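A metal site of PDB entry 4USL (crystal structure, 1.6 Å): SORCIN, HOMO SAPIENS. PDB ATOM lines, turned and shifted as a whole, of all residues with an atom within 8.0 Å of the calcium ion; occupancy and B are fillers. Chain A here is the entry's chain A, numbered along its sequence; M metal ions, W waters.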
ATOM      1  N   PHE A 109      -4.065  25.154 -17.364  1.00  0.00           N
ATOM      2  CA  PHE A 109      -5.225  25.234 -18.285  1.00  0.00           C
ATOM      3  C   PHE A 109      -5.239  26.534 -19.096  1.00  0.00           C
ATOM      4  O   PHE A 109      -5.322  26.507 -20.333  1.00  0.00           O
ATOM      5  CB  PHE A 109      -6.528  25.099 -17.480  1.00  0.00           C
ATOM      6  CG  PHE A 109      -7.812  25.120 -18.293  1.00  0.00           C
ATOM      7  CD1 PHE A 109      -8.363  23.942 -18.771  1.00  0.00           C
ATOM      8  CD2 PHE A 109      -8.504  26.305 -18.539  1.00  0.00           C
ATOM      9  CE1 PHE A 109      -9.571  23.931 -19.444  1.00  0.00           C
ATOM     10  CE2 PHE A 109      -9.695  26.310 -19.249  1.00  0.00           C
ATOM     11  CZ  PHE A 109     -10.222  25.116 -19.705  1.00  0.00           C
ATOM     12  N   ILE A 110      -5.160  27.654 -18.387  1.00  0.00           N
ATOM     13  CA  ILE A 110      -5.116  28.964 -19.026  1.00  0.00           C
ATOM     14  C   ILE A 110      -3.995  28.975 -20.070  1.00  0.00           C
ATOM     15  O   ILE A 110      -4.191  29.442 -21.209  1.00  0.00           O
ATOM     16  CB  ILE A 110      -4.963  30.113 -17.989  1.00  0.00           C
ATOM     17  CG1 ILE A 110      -6.281  30.279 -17.222  1.00  0.00           C
ATOM     18  CG2 ILE A 110      -4.638  31.414 -18.705  1.00  0.00           C
ATOM     19  CD1 ILE A 110      -6.208  31.251 -16.037  1.00  0.00           C
ATOM     20  N   PHE A 112      -2.607  26.616 -21.900  1.00  0.00           N
ATOM     21  CA  PHE A 112      -2.824  25.863 -23.144  1.00  0.00           C
ATOM     22  C   PHE A 112      -4.074  26.277 -23.912  1.00  0.00           C
ATOM     23  O   PHE A 112      -4.253  25.886 -25.061  1.00  0.00           O
ATOM     24  CB  PHE A 112      -2.691  24.359 -22.908  1.00  0.00           C
ATOM     25  CG  PHE A 112      -1.268  23.935 -22.658  1.00  0.00           C
ATOM     26  CD1 PHE A 112      -0.364  23.824 -23.712  1.00  0.00           C
ATOM     27  CD2 PHE A 112      -0.798  23.736 -21.360  1.00  0.00           C
ATOM     28  CE1 PHE A 112       0.952  23.467 -23.481  1.00  0.00           C
ATOM     29  CE2 PHE A 112       0.512  23.387 -21.126  1.00  0.00           C
ATOM     30  CZ  PHE A 112       1.405  23.255 -22.188  1.00  0.00           C
ATOM     31  N   ASP A 113      -4.877  27.153 -23.286  1.00  0.00           N
ATOM     32  CA  ASP A 113      -6.059  27.734 -23.898  1.00  0.00           C
ATOM     33  C   ASP A 113      -5.650  28.979 -24.672  1.00  0.00           C
ATOM     34  O   ASP A 113      -6.015  30.094 -24.307  1.00  0.00           O
ATOM     35  CB  ASP A 113      -7.080  28.122 -22.813  1.00  0.00           C
ATOM     36  CG  ASP A 113      -8.360  28.723 -23.385  1.00  0.00           C
ATOM     37  OD1 ASP A 113      -8.625  28.607 -24.601  1.00  0.00           O
ATOM     38  OD2 ASP A 113      -9.114  29.320 -22.593  1.00  0.00           O
ATOM     39  N   THR A 114      -4.889  28.773 -25.741  1.00  0.00           N
ATOM     40  CA  THR A 114      -4.220  29.880 -26.431  1.00  0.00           C
ATOM     41  C   THR A 114      -5.159  30.810 -27.178  1.00  0.00           C
ATOM     42  O   THR A 114      -4.772  31.937 -27.478  1.00  0.00           O
ATOM     43  CB  THR A 114      -3.102  29.361 -27.359  1.00  0.00           C
ATOM     44  OG1 THR A 114      -3.637  28.368 -28.249  1.00  0.00           O
ATOM     45  CG2 THR A 114      -1.981  28.734 -26.533  1.00  0.00           C
ATOM     46  N   ASP A 115      -6.390  30.388 -27.461  1.00  0.00           N
ATOM     47  CA  ASP A 115      -7.377  31.316 -28.039  1.00  0.00           C
ATOM     48  C   ASP A 115      -8.310  31.915 -26.963  1.00  0.00           C
ATOM     49  O   ASP A 115      -9.302  32.559 -27.279  1.00  0.00           O
ATOM     50  CB  ASP A 115      -8.157  30.657 -29.210  1.00  0.00           C
ATOM     51  CG  ASP A 115      -9.142  29.593 -28.771  1.00  0.00           C
ATOM     52  OD1 ASP A 115      -9.158  29.236 -27.575  1.00  0.00           O
ATOM     53  OD2 ASP A 115      -9.902  29.080 -29.639  1.00  0.00           O
ATOM     54  N   ARG A 116      -7.984  31.679 -25.687  1.00  0.00           N
ATOM     55  CA  ARG A 116      -8.767  32.207 -24.555  1.00  0.00           C
ATOM     56  C   ARG A 116     -10.282  31.973 -24.652  1.00  0.00           C
ATOM     57  O   ARG A 116     -11.087  32.845 -24.326  1.00  0.00           O
ATOM     58  CB  ARG A 116      -8.448  33.699 -24.386  1.00  0.00           C
ATOM     59  CG  ARG A 116      -7.006  33.915 -23.930  1.00  0.00           C
ATOM     60  CD  ARG A 116      -6.476  35.291 -24.312  1.00  0.00           C
ATOM     61  NE  ARG A 116      -7.161  36.365 -23.601  1.00  0.00           N
ATOM     62  CZ  ARG A 116      -6.825  36.834 -22.400  1.00  0.00           C
ATOM     63  NH1 ARG A 116      -5.799  36.339 -21.722  1.00  0.00           N
ATOM     64  NH2 ARG A 116      -7.528  37.827 -21.870  1.00  0.00           N
ATOM     65  N   SER A 117     -10.665  30.766 -25.067  1.00  0.00           N
ATOM     66  CA  SER A 117     -12.082  30.374 -25.180  1.00  0.00           C
ATOM     67  C   SER A 117     -12.673  29.930 -23.843  1.00  0.00           C
ATOM     68  O   SER A 117     -13.882  29.733 -23.733  1.00  0.00           O
ATOM     69  CB  SER A 117     -12.254  29.269 -26.228  1.00  0.00           C
ATOM     70  OG  SER A 117     -11.579  28.069 -25.848  1.00  0.00           O
ATOM     71  N   GLY A 118     -11.820  29.746 -22.831  1.00  0.00           N
ATOM     72  CA  GLY A 118     -12.230  29.152 -21.552  1.00  0.00           C
ATOM     73  C   GLY A 118     -12.376  27.651 -21.627  1.00  0.00           C
ATOM     74  O   GLY A 118     -12.846  27.019 -20.661  1.00  0.00           O
ATOM     75  N   THR A 119     -11.992  27.076 -22.769  1.00  0.00           N
ATOM     76  CA  THR A 119     -11.984  25.636 -22.996  1.00  0.00           C
ATOM     77  C   THR A 119     -10.701  25.251 -23.753  1.00  0.00           C
ATOM     78  O   THR A 119     -10.093  26.079 -24.481  1.00  0.00           O
ATOM     79  CB  THR A 119     -13.203  25.138 -23.815  1.00  0.00           C
ATOM     80  OG1 THR A 119     -13.239  25.792 -25.090  1.00  0.00           O
ATOM     81  CG2 THR A 119     -14.524  25.419 -23.094  1.00  0.00           C
ATOM     82  N   VAL A 120     -10.320  23.992 -23.564  1.00  0.00           N
ATOM     83  CA  VAL A 120      -9.172  23.379 -24.241  1.00  0.00           C
ATOM     84  C   VAL A 120      -9.725  22.484 -25.333  1.00  0.00           C
ATOM     85  O   VAL A 120     -10.380  21.464 -25.061  1.00  0.00           O
ATOM     86  CB  VAL A 120      -8.335  22.551 -23.244  1.00  0.00           C
ATOM     87  CG1 VAL A 120      -7.298  21.667 -23.950  1.00  0.00           C
ATOM     88  CG2 VAL A 120      -7.641  23.469 -22.238  1.00  0.00           C
ATOM     89  N   ASP A 121      -9.420  22.831 -26.587  1.00  0.00           N
ATOM     90  CA  ASP A 121      -9.835  22.005 -27.717  1.00  0.00           C
ATOM     91  C   ASP A 121      -8.851  20.841 -27.969  1.00  0.00           C
ATOM     92  O   ASP A 121      -7.803  20.721 -27.297  1.00  0.00           O
ATOM     93  CB  ASP A 121     -10.110  22.918 -28.946  1.00  0.00           C
ATOM     94  CG  ASP A 121      -8.857  23.531 -29.550  1.00  0.00           C
ATOM     95  OD1 ASP A 121      -7.843  22.827 -29.688  1.00  0.00           O
ATOM     96  OD2 ASP A 121      -8.914  24.723 -29.922  1.00  0.00           O
ATOM     97  N   PRO A 122      -9.162  19.968 -28.927  1.00  0.00           N
ATOM     98  CA  PRO A 122      -8.310  18.796 -29.108  1.00  0.00           C
ATOM     99  C   PRO A 122      -6.881  19.120 -29.552  1.00  0.00           C
ATOM    100  O   PRO A 122      -5.949  18.410 -29.175  1.00  0.00           O
ATOM    101  CB  PRO A 122      -9.063  17.952 -30.151  1.00  0.00           C
ATOM    102  CG  PRO A 122     -10.467  18.412 -30.040  1.00  0.00           C
ATOM    103  CD  PRO A 122     -10.415  19.858 -29.697  1.00  0.00           C
ATOM    104  N   GLU A 124      -5.283  21.984 -28.766  1.00  0.00           N
ATOM    105  CA  GLU A 124      -4.708  22.530 -27.534  1.00  0.00           C
ATOM    106  C   GLU A 124      -4.350  21.438 -26.542  1.00  0.00           C
ATOM    107  O   GLU A 124      -3.284  21.469 -25.920  1.00  0.00           O
ATOM    108  CB  GLU A 124      -5.684  23.531 -26.908  1.00  0.00           C
ATOM    109  CG  GLU A 124      -5.836  24.835 -27.720  1.00  0.00           C
ATOM    110  CD  GLU A 124      -6.961  25.696 -27.185  1.00  0.00           C
ATOM    111  OE1 GLU A 124      -7.868  25.178 -26.526  1.00  0.00           O
ATOM    112  OE2 GLU A 124      -6.998  26.922 -27.423  1.00  0.00           O
ATOM    113  N   LEU A 125      -5.203  20.432 -26.429  1.00  0.00           N
ATOM    114  CA  LEU A 125      -4.927  19.279 -25.570  1.00  0.00           C
ATOM    115  C   LEU A 125      -3.684  18.482 -26.038  1.00  0.00           C
ATOM    116  O   LEU A 125      -2.823  18.082 -25.237  1.00  0.00           O
ATOM    117  CB  LEU A 125      -6.155  18.360 -25.468  1.00  0.00           C
ATOM    118  CG  LEU A 125      -5.954  17.153 -24.509  1.00  0.00           C
ATOM    119  CD1 LEU A 125      -5.795  17.598 -23.059  1.00  0.00           C
ATOM    120  CD2 LEU A 125      -7.071  16.123 -24.608  1.00  0.00           C
ATOM    121  N   LYS A 153     -14.569  20.696 -26.857  1.00  0.00           N
ATOM    122  CA  LYS A 153     -14.145  21.828 -26.001  1.00  0.00           C
ATOM    123  C   LYS A 153     -14.189  21.489 -24.503  1.00  0.00           C
ATOM    124  O   LYS A 153     -15.235  21.478 -23.874  1.00  0.00           O
ATOM    125  CB  LYS A 153     -14.996  23.069 -26.288  1.00  0.00           C
ATOM    126  CG  LYS A 153     -15.085  23.439 -27.776  1.00  0.00           C
ATOM    127  CD  LYS A 153     -13.720  23.466 -28.462  1.00  0.00           C
ATOM    128  CE  LYS A 153     -13.838  23.456 -29.985  1.00  0.00           C
ATOM    129  NZ  LYS A 153     -14.375  24.732 -30.520  1.00  0.00           N
ATOM    130  N   ILE A 154     -13.014  21.229 -23.931  1.00  0.00           N
ATOM    131  CA  ILE A 154     -12.881  20.661 -22.581  1.00  0.00           C
ATOM    132  C   ILE A 154     -12.892  21.771 -21.537  1.00  0.00           C
ATOM    133  O   ILE A 154     -12.086  22.711 -21.593  1.00  0.00           O
ATOM    134  CB  ILE A 154     -11.565  19.857 -22.466  1.00  0.00           C
ATOM    135  CG1 ILE A 154     -11.491  18.801 -23.606  1.00  0.00           C
ATOM    136  CG2 ILE A 154     -11.399  19.194 -21.091  1.00  0.00           C
ATOM    137  CD1 ILE A 154     -10.129  18.218 -23.783  1.00  0.00           C
HETATM  138 CA    CA M   1      -9.350  27.206 -26.314  1.00  0.00          CA
HETATM  139  O   HOH W   1     -10.412  26.407 -28.137  1.00  0.00           O
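The side-chain carboxylate of Asp 113 sits close to the backbone NH of Arg 116 (3.3 Å).
The side-chain carboxylate of Asp 113 is in hydrogen-bond range of the backbone NH of Gly 118 (2.7 Å).
The backbone NH of Glu 124 sits at hydrogen-bond distance from the side-chain carboxylate of Asp 121 (2.8 Å).
The side-chain carboxylate (OE2) of Glu 124 lies close to the backbone NH (N) of Thr 114, at 3.3 Å.
Water W1 is bound to the calcium ion (2.3 Å).
The calcium ion is bound by the backbone carbonyl oxygen (O) of Thr 119 (2.3 Å).
The side-chain carboxylate (OD1) of Asp 113 binds the calcium ion, 2.3 Å away.
The side-chain carboxylate (OD1) of Asp 115 is bound to the calcium ion, at 2.4 Å.
OG of Ser 117 binds the calcium ion (2.4 Å).
OE1 of Glu 124 binds the calcium ion, at 2.5 Å.
The side-chain carboxylate (OE2) of Glu 124 is bound to the calcium ion.
Water W1 lies within hydrogen-bond range of the side-chain carboxylate (OD2) of Asp 121 and the side-chain carboxylate (OD2) of Asp 115.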
